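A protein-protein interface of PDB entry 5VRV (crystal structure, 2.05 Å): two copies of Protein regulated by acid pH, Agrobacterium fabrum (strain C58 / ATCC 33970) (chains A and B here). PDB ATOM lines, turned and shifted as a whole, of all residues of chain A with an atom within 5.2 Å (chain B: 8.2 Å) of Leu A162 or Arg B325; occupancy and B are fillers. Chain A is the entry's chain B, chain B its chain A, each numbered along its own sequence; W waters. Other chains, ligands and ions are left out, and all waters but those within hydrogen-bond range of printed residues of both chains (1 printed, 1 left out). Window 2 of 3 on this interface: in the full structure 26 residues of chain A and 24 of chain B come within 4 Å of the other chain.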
ATOM      1  N   SER A 158       6.893  38.098 -11.388  1.00  0.00           N
ATOM      2  CA  SER A 158       7.587  36.845 -11.701  1.00  0.00           C
ATOM      3  C   SER A 158       8.636  36.511 -10.627  1.00  0.00           C
ATOM      4  O   SER A 158       8.709  35.356 -10.149  1.00  0.00           O
ATOM      5  CB  SER A 158       8.253  36.908 -13.089  1.00  0.00           C
ATOM      6  OG  SER A 158       8.864  35.666 -13.406  1.00  0.00           O
ATOM      7  N   ASP A 159       9.442  37.506 -10.249  1.00  0.00           N
ATOM      8  CA  ASP A 159      10.464  37.303  -9.206  1.00  0.00           C
ATOM      9  C   ASP A 159       9.816  36.960  -7.852  1.00  0.00           C
ATOM     10  O   ASP A 159      10.351  36.124  -7.114  1.00  0.00           O
ATOM     11  CB  ASP A 159      11.398  38.518  -9.070  1.00  0.00           C
ATOM     12  CG  ASP A 159      12.297  38.714 -10.296  1.00  0.00           C
ATOM     13  OD1 ASP A 159      12.331  37.821 -11.173  1.00  0.00           O
ATOM     14  OD2 ASP A 159      12.975  39.762 -10.377  1.00  0.00           O
ATOM     15  N   GLY A 160       8.673  37.582  -7.539  1.00  0.00           N
ATOM     16  CA  GLY A 160       7.941  37.276  -6.291  1.00  0.00           C
ATOM     17  C   GLY A 160       7.400  35.835  -6.279  1.00  0.00           C
ATOM     18  O   GLY A 160       7.372  35.174  -5.251  1.00  0.00           O
ATOM     19  N   TRP A 161       6.995  35.343  -7.445  1.00  0.00           N
ATOM     20  CA  TRP A 161       6.473  33.974  -7.589  1.00  0.00           C
ATOM     21  C   TRP A 161       7.580  32.939  -7.386  1.00  0.00           C
ATOM     22  O   TRP A 161       7.364  31.910  -6.732  1.00  0.00           O
ATOM     23  CB  TRP A 161       5.855  33.818  -8.976  1.00  0.00           C
ATOM     24  CG  TRP A 161       5.210  32.516  -9.288  1.00  0.00           C
ATOM     25  CD1 TRP A 161       3.923  32.172  -9.038  1.00  0.00           C
ATOM     26  CD2 TRP A 161       5.795  31.399  -9.972  1.00  0.00           C
ATOM     27  NE1 TRP A 161       3.660  30.918  -9.515  1.00  0.00           N
ATOM     28  CE2 TRP A 161       4.797  30.410 -10.082  1.00  0.00           C
ATOM     29  CE3 TRP A 161       7.062  31.139 -10.503  1.00  0.00           C
ATOM     30  CZ2 TRP A 161       5.023  29.173 -10.703  1.00  0.00           C
ATOM     31  CZ3 TRP A 161       7.293  29.898 -11.115  1.00  0.00           C
ATOM     32  CH2 TRP A 161       6.272  28.935 -11.212  1.00  0.00           C
ATOM     33  N   LEU A 162       8.752  33.212  -7.963  1.00  0.00           N
ATOM     34  CA  LEU A 162       9.892  32.310  -7.845  1.00  0.00           C
ATOM     35  C   LEU A 162      10.312  32.248  -6.382  1.00  0.00           C
ATOM     36  O   LEU A 162      10.603  31.178  -5.869  1.00  0.00           O
ATOM     37  CB  LEU A 162      11.059  32.747  -8.727  1.00  0.00           C
ATOM     38  CG  LEU A 162      10.915  32.638 -10.257  1.00  0.00           C
ATOM     39  CD1 LEU A 162      12.020  33.408 -10.984  1.00  0.00           C
ATOM     40  CD2 LEU A 162      10.892  31.184 -10.719  1.00  0.00           C
ATOM     41  N   ALA A 163      10.329  33.400  -5.720  1.00  0.00           N
ATOM     42  CA  ALA A 163      10.683  33.464  -4.307  1.00  0.00           C
ATOM     43  C   ALA A 163       9.597  32.788  -3.435  1.00  0.00           C
ATOM     44  O   ALA A 163       9.917  31.985  -2.554  1.00  0.00           O
ATOM     45  CB  ALA A 163      10.915  34.906  -3.870  1.00  0.00           C
ATOM     46  N   HIS A 164       8.327  33.063  -3.730  1.00  0.00           N
ATOM     47  CA  HIS A 164       7.219  32.484  -2.957  1.00  0.00           C
ATOM     48  C   HIS A 164       7.206  30.973  -3.023  1.00  0.00           C
ATOM     49  O   HIS A 164       7.030  30.322  -2.002  1.00  0.00           O
ATOM     50  CB  HIS A 164       5.857  33.036  -3.408  1.00  0.00           C
ATOM     51  CG  HIS A 164       4.690  32.406  -2.710  1.00  0.00           C
ATOM     52  ND1 HIS A 164       4.388  32.658  -1.389  1.00  0.00           N
ATOM     53  CD2 HIS A 164       3.740  31.549  -3.154  1.00  0.00           C
ATOM     54  CE1 HIS A 164       3.304  31.983  -1.048  1.00  0.00           C
ATOM     55  NE2 HIS A 164       2.890  31.303  -2.101  1.00  0.00           N
ATOM     56  N   HIS A 165       7.384  30.408  -4.214  1.00  0.00           N
ATOM     57  CA  HIS A 165       7.407  28.944  -4.346  1.00  0.00           C
ATOM     58  C   HIS A 165       8.829  28.339  -4.132  1.00  0.00           C
ATOM     59  O   HIS A 165       8.996  27.135  -4.228  1.00  0.00           O
ATOM     60  CB  HIS A 165       6.813  28.520  -5.692  1.00  0.00           C
ATOM     61  CG  HIS A 165       5.370  28.902  -5.867  1.00  0.00           C
ATOM     62  ND1 HIS A 165       4.328  28.112  -5.427  1.00  0.00           N
ATOM     63  CD2 HIS A 165       4.794  29.990  -6.436  1.00  0.00           C
ATOM     64  CE1 HIS A 165       3.179  28.697  -5.714  1.00  0.00           C
ATOM     65  NE2 HIS A 165       3.435  29.838  -6.328  1.00  0.00           N
ATOM     66  N   ASN A 166       9.830  29.177  -3.844  1.00  0.00           N
ATOM     67  CA  ASN A 166      11.220  28.731  -3.625  1.00  0.00           C
ATOM     68  C   ASN A 166      11.664  27.824  -4.791  1.00  0.00           C
ATOM     69  O   ASN A 166      12.249  26.750  -4.589  1.00  0.00           O
ATOM     70  CB  ASN A 166      11.333  28.004  -2.275  1.00  0.00           C
ATOM     71  CG  ASN A 166      12.771  27.737  -1.859  1.00  0.00           C
ATOM     72  OD1 ASN A 166      13.694  28.413  -2.297  1.00  0.00           O
ATOM     73  ND2 ASN A 166      12.959  26.766  -0.969  1.00  0.00           N
ATOM     74  N   THR A 167      11.403  28.278  -6.014  1.00  0.00           N
ATOM     75  CA  THR A 167      11.720  27.486  -7.190  1.00  0.00           C
ATOM     76  C   THR A 167      12.577  28.249  -8.201  1.00  0.00           C
ATOM     77  O   THR A 167      12.854  29.459  -8.046  1.00  0.00           O
ATOM     78  CB  THR A 167      10.417  26.946  -7.823  1.00  0.00           C
ATOM     79  OG1 THR A 167      10.718  25.916  -8.756  1.00  0.00           O
ATOM     80  CG2 THR A 167       9.594  28.061  -8.505  1.00  0.00           C
ATOM     81  N   ARG A 168      12.992  27.526  -9.234  1.00  0.00           N
ATOM     82  CA  ARG A 168      13.841  28.072 -10.291  1.00  0.00           C
ATOM     83  C   ARG A 168      13.183  27.934 -11.633  1.00  0.00           C
ATOM     84  O   ARG A 168      12.284  27.126 -11.808  1.00  0.00           O
ATOM     85  CB  ARG A 168      15.179  27.338 -10.317  1.00  0.00           C
ATOM     86  CG  ARG A 168      16.014  27.527  -9.056  1.00  0.00           C
ATOM     87  CD  ARG A 168      17.285  26.695  -9.144  1.00  0.00           C
ATOM     88  NE  ARG A 168      18.189  27.179 -10.189  1.00  0.00           N
ATOM     89  CZ  ARG A 168      19.191  26.482 -10.710  1.00  0.00           C
ATOM     90  NH1 ARG A 168      19.408  25.212 -10.338  1.00  0.00           N
ATOM     91  NH2 ARG A 168      19.963  27.042 -11.645  1.00  0.00           N
ATOM     92  N   GLU A 169      13.631  28.745 -12.581  1.00  0.00           N
ATOM     93  CA  GLU A 169      13.122  28.677 -13.941  1.00  0.00           C
ATOM     94  C   GLU A 169      13.434  27.306 -14.571  1.00  0.00           C
ATOM     95  O   GLU A 169      14.388  26.624 -14.159  1.00  0.00           O
ATOM     96  CB  GLU A 169      13.765  29.787 -14.793  1.00  0.00           C
ATOM     97  CG  GLU A 169      13.353  31.205 -14.464  1.00  0.00           C
ATOM     98  CD  GLU A 169      11.929  31.532 -14.863  1.00  0.00           C
ATOM     99  OE1 GLU A 169      11.196  30.625 -15.278  1.00  0.00           O
ATOM    100  OE2 GLU A 169      11.534  32.725 -14.792  1.00  0.00           O
ATOM    101  N   ARG A 217       1.735  32.834 -13.844  1.00  0.00           N
ATOM    102  CA  ARG A 217       2.184  33.200 -12.502  1.00  0.00           C
ATOM    103  C   ARG A 217       1.265  34.160 -11.750  1.00  0.00           C
ATOM    104  O   ARG A 217       0.915  35.217 -12.241  1.00  0.00           O
ATOM    105  CB  ARG A 217       3.613  33.727 -12.577  1.00  0.00           C
ATOM    106  CG  ARG A 217       4.536  32.655 -13.120  1.00  0.00           C
ATOM    107  CD  ARG A 217       5.980  33.055 -13.277  1.00  0.00           C
ATOM    108  NE  ARG A 217       6.691  31.926 -13.838  1.00  0.00           N
ATOM    109  CZ  ARG A 217       7.990  31.882 -14.089  1.00  0.00           C
ATOM    110  NH1 ARG A 217       8.773  32.924 -13.849  1.00  0.00           N
ATOM    111  NH2 ARG A 217       8.504  30.765 -14.586  1.00  0.00           N
ATOM    112  N   MET B  26      25.085  26.713   1.720  1.00  0.00           N
ATOM    113  CA  MET B  26      24.323  27.244   0.583  1.00  0.00           C
ATOM    114  C   MET B  26      22.918  27.601   1.015  1.00  0.00           C
ATOM    115  O   MET B  26      22.268  28.407   0.376  1.00  0.00           O
ATOM    116  CB  MET B  26      24.286  26.250  -0.577  1.00  0.00           C
ATOM    117  CG  MET B  26      25.471  26.460  -1.519  1.00  0.00           C
ATOM    118  SD  MET B  26      25.118  27.939  -2.770  1.00  0.00           S
ATOM    119  CE  MET B  26      23.390  27.403  -3.554  1.00  0.00           C
ATOM    120  N   GLY B  27      22.438  26.994   2.097  1.00  0.00           N
ATOM    121  CA  GLY B  27      21.090  27.290   2.600  1.00  0.00           C
ATOM    122  C   GLY B  27      19.947  26.771   1.746  1.00  0.00           C
ATOM    123  O   GLY B  27      18.800  27.188   1.923  1.00  0.00           O
ATOM    124  N   ASP B  28      20.249  25.866   0.820  1.00  0.00           N
ATOM    125  CA  ASP B  28      19.228  25.311  -0.049  1.00  0.00           C
ATOM    126  C   ASP B  28      18.685  23.977   0.458  1.00  0.00           C
ATOM    127  O   ASP B  28      17.790  23.419  -0.146  1.00  0.00           O
ATOM    128  CB  ASP B  28      19.760  25.150  -1.484  1.00  0.00           C
ATOM    129  CG  ASP B  28      20.876  24.117  -1.607  1.00  0.00           C
ATOM    130  OD1 ASP B  28      21.615  23.875  -0.635  1.00  0.00           O
ATOM    131  OD2 ASP B  28      21.031  23.558  -2.715  1.00  0.00           O
ATOM    132  N   ARG B 168      23.651  26.101 -16.667  1.00  0.00           N
ATOM    133  CA  ARG B 168      23.058  26.809 -15.530  1.00  0.00           C
ATOM    134  C   ARG B 168      23.595  26.249 -14.239  1.00  0.00           C
ATOM    135  O   ARG B 168      24.184  25.165 -14.217  1.00  0.00           O
ATOM    136  CB  ARG B 168      21.537  26.684 -15.549  1.00  0.00           C
ATOM    137  CG  ARG B 168      20.856  27.250 -16.789  1.00  0.00           C
ATOM    138  CD  ARG B 168      19.382  26.865 -16.778  1.00  0.00           C
ATOM    139  NE  ARG B 168      18.643  27.509 -15.696  1.00  0.00           N
ATOM    140  CZ  ARG B 168      17.483  27.094 -15.186  1.00  0.00           C
ATOM    141  NH1 ARG B 168      16.901  25.958 -15.579  1.00  0.00           N
ATOM    142  NH2 ARG B 168      16.925  27.793 -14.199  1.00  0.00           N
ATOM    143  N   LYS B 170      23.697  24.658 -10.445  1.00  0.00           N
ATOM    144  CA  LYS B 170      23.136  23.449  -9.848  1.00  0.00           C
ATOM    145  C   LYS B 170      22.786  23.757  -8.380  1.00  0.00           C
ATOM    146  O   LYS B 170      22.930  24.890  -7.922  1.00  0.00           O
ATOM    147  CB  LYS B 170      24.139  22.294  -9.923  1.00  0.00           C
ATOM    148  CG  LYS B 170      24.606  21.911 -11.311  1.00  0.00           C
ATOM    149  CD  LYS B 170      23.519  21.304 -12.156  1.00  0.00           C
ATOM    150  CE  LYS B 170      24.071  20.848 -13.508  1.00  0.00           C
ATOM    151  NZ  LYS B 170      24.681  21.914 -14.348  1.00  0.00           N
ATOM    152  N   ARG B 171      22.314  22.734  -7.667  1.00  0.00           N
ATOM    153  CA  ARG B 171      21.926  22.820  -6.269  1.00  0.00           C
ATOM    154  C   ARG B 171      22.192  21.472  -5.565  1.00  0.00           C
ATOM    155  O   ARG B 171      22.673  20.515  -6.185  1.00  0.00           O
ATOM    156  CB  ARG B 171      20.422  23.090  -6.169  1.00  0.00           C
ATOM    157  CG  ARG B 171      19.925  24.453  -6.596  1.00  0.00           C
ATOM    158  CD  ARG B 171      20.376  25.544  -5.659  1.00  0.00           C
ATOM    159  NE  ARG B 171      19.777  26.829  -6.016  1.00  0.00           N
ATOM    160  CZ  ARG B 171      20.260  27.704  -6.904  1.00  0.00           C
ATOM    161  NH1 ARG B 171      21.366  27.458  -7.597  1.00  0.00           N
ATOM    162  NH2 ARG B 171      19.604  28.844  -7.112  1.00  0.00           N
ATOM    163  N   ALA B 176      26.664  26.956  -5.792  1.00  0.00           N
ATOM    164  CA  ALA B 176      26.428  27.881  -6.896  1.00  0.00           C
ATOM    165  C   ALA B 176      27.133  29.186  -6.613  1.00  0.00           C
ATOM    166  O   ALA B 176      27.540  29.430  -5.478  1.00  0.00           O
ATOM    167  CB  ALA B 176      24.947  28.119  -7.065  1.00  0.00           C
ATOM    168  N   GLU B 178      26.837  32.252  -5.519  1.00  0.00           N
ATOM    169  CA  GLU B 178      25.966  33.172  -4.791  1.00  0.00           C
ATOM    170  C   GLU B 178      26.956  33.937  -3.913  1.00  0.00           C
ATOM    171  O   GLU B 178      27.651  33.317  -3.110  1.00  0.00           O
ATOM    172  CB  GLU B 178      24.920  32.399  -3.980  1.00  0.00           C
ATOM    173  CG  GLU B 178      23.818  33.254  -3.360  1.00  0.00           C
ATOM    174  CD  GLU B 178      24.285  34.058  -2.161  1.00  0.00           C
ATOM    175  OE1 GLU B 178      25.196  33.574  -1.456  1.00  0.00           O
ATOM    176  OE2 GLU B 178      23.725  35.156  -1.908  1.00  0.00           O
ATOM    177  N   GLY B 322      17.721  21.299 -11.114  1.00  0.00           N
ATOM    178  CA  GLY B 322      16.853  22.468 -10.993  1.00  0.00           C
ATOM    179  C   GLY B 322      16.798  22.757  -9.517  1.00  0.00           C
ATOM    180  O   GLY B 322      17.667  23.420  -8.980  1.00  0.00           O
ATOM    181  N   GLY B 323      15.774  22.231  -8.866  1.00  0.00           N
ATOM    182  CA  GLY B 323      15.656  22.365  -7.431  1.00  0.00           C
ATOM    183  C   GLY B 323      15.175  23.687  -6.890  1.00  0.00           C
ATOM    184  O   GLY B 323      14.518  24.471  -7.581  1.00  0.00           O
ATOM    185  N   VAL B 324      15.534  23.931  -5.642  1.00  0.00           N
ATOM    186  CA  VAL B 324      15.069  25.112  -4.928  1.00  0.00           C
ATOM    187  C   VAL B 324      15.835  26.377  -5.263  1.00  0.00           C
ATOM    188  O   VAL B 324      16.992  26.326  -5.673  1.00  0.00           O
ATOM    189  CB  VAL B 324      15.084  24.901  -3.383  1.00  0.00           C
ATOM    190  CG1 VAL B 324      14.239  23.690  -2.988  1.00  0.00           C
ATOM    191  CG2 VAL B 324      16.492  24.750  -2.843  1.00  0.00           C
ATOM    192  N   ARG B 325      15.177  27.511  -5.080  1.00  0.00           N
ATOM    193  CA  ARG B 325      15.814  28.785  -5.326  1.00  0.00           C
ATOM    194  C   ARG B 325      16.936  28.947  -4.293  1.00  0.00           C
ATOM    195  O   ARG B 325      18.070  29.305  -4.636  1.00  0.00           O
ATOM    196  CB  ARG B 325      14.796  29.909  -5.208  1.00  0.00           C
ATOM    197  CG  ARG B 325      15.339  31.256  -5.616  1.00  0.00           C
ATOM    198  CD  ARG B 325      14.240  32.289  -5.742  1.00  0.00           C
ATOM    199  NE  ARG B 325      14.713  33.419  -6.534  1.00  0.00           N
ATOM    200  CZ  ARG B 325      14.827  33.415  -7.867  1.00  0.00           C
ATOM    201  NH1 ARG B 325      14.537  32.325  -8.591  1.00  0.00           N
ATOM    202  NH2 ARG B 325      15.266  34.494  -8.484  1.00  0.00           N
ATOM    203  N   GLY B 326      16.612  28.635  -3.038  1.00  0.00           N
ATOM    204  CA  GLY B 326      17.572  28.723  -1.928  1.00  0.00           C
ATOM    205  C   GLY B 326      17.644  30.107  -1.364  1.00  0.00           C
ATOM    206  O   GLY B 326      16.763  30.916  -1.604  1.00  0.00           O
ATOM    207  N   VAL B 327      18.687  30.370  -0.588  1.00  0.00           N
ATOM    208  CA  VAL B 327      18.904  31.682   0.010  1.00  0.00           C
ATOM    209  C   VAL B 327      19.652  32.569  -0.998  1.00  0.00           C
ATOM    210  O   VAL B 327      20.640  32.137  -1.602  1.00  0.00           O
ATOM    211  CB  VAL B 327      19.708  31.582   1.336  1.00  0.00           C
ATOM    212  CG1 VAL B 327      20.010  32.974   1.899  1.00  0.00           C
ATOM    213  CG2 VAL B 327      18.949  30.745   2.359  1.00  0.00           C
ATOM    214  N   ILE B 328      19.159  33.797  -1.182  1.00  0.00           N
ATOM    215  CA  ILE B 328      19.762  34.781  -2.099  1.00  0.00           C
ATOM    216  C   ILE B 328      19.865  36.155  -1.421  1.00  0.00           C
ATOM    217  O   ILE B 328      18.946  36.577  -0.708  1.00  0.00           O
ATOM    218  CB  ILE B 328      18.957  34.923  -3.421  1.00  0.00           C
ATOM    219  CG1 ILE B 328      18.837  33.563  -4.126  1.00  0.00           C
ATOM    220  CG2 ILE B 328      19.613  35.955  -4.350  1.00  0.00           C
ATOM    221  CD1 ILE B 328      18.102  33.607  -5.450  1.00  0.00           C
HETATM  222  O   HOH W   1      13.276  24.334  -9.853  1.00  0.00           O
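N of Arg B325 is in hydrogen-bond range of O of Asn A166 (3.1 Å). N of Gly B326 sits at hydrogen-bond distance from OD1 of Asn A166 (3.0 Å). NH2 of Arg B168 sits at hydrogen-bond distance from O of Glu A169 (2.8 Å). O of Thr A167 sits at hydrogen-bond distance from NH1 of Arg B325, at 3.4 Å. The backbone carbonyl oxygen (O) of Gly B322 sits at hydrogen-bond distance from the guanidinium group (NH1) of Arg A168 (2.8 Å).
NE of Arg B171 lies within hydrogen-bond range of O of Val B324, 2.9 Å away. The guanidinium group of Arg A217 lies within salt-bridge range of the side-chain carboxylate of Glu A169 (2.8 Å). O of Arg B325 sits at hydrogen-bond distance from NH2 of Arg B171, 2.9 Å away. The backbone carbonyl oxygen of Leu A162 is in hydrogen-bond range of the backbone NH of Thr A167 (3.0 Å). The side-chain amino group (NZ) of Lys B170 is in hydrogen-bond range of the backbone carbonyl oxygen (O) of Arg B168.
Among the printed residues, pairs that only touch across the chains: Leu A162 with Arg B325 (3.5 Å), Asn A166 with Val B324 (3.3 Å), Arg A168 with Arg B171 (3.8 Å), Arg A168 with Gly B323 (3.7 Å), Arg A168 with Val B324 (3.5 Å) and Arg A168 with Arg B325 (3.9 Å).
Trp A161 touches none of the printed residues of chain B. Arg A217 touches none of the printed residues of chain B. Of the printed residues of chain A, Arg B168 touches Glu A169 (2.8 Å). Of the printed residues of chain A, Arg B325 touches Leu A162 (3.5 Å), Asn A166 (3.1 Å), Thr A167 (3.4 Å) and Arg A168 (3.9 Å). Of the printed residues of chain A, Gly B326 touches Asn A166 (3.0 Å). The nearest printed residue of chain A that does not touch Arg B325 is Ala A163 (4.01 Å).
Printed residues of chain B that touch a printed residue of chain A: Arg B168, Arg B171, Gly B322, Gly B323, Val B324, Arg B325 and Gly B326. Hydrophobic or aromatic side chains of chain B within 4 Å of the printed part of chain A: Val B324. Of the 13 printed residues of chain A, 5 touch a printed residue of chain B. Among the printed residues, no Asp or Glu carboxylate lies within 4 Å of a Lys or Arg side-chain nitrogen of the other chain.
Position printed for both chains: 168.
Water W1 lies within hydrogen-bond range of O of Gly B323 (2.6 Å), OG1 of Thr A167 (3.2 Å) and N of Arg A168 (3.3 Å).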
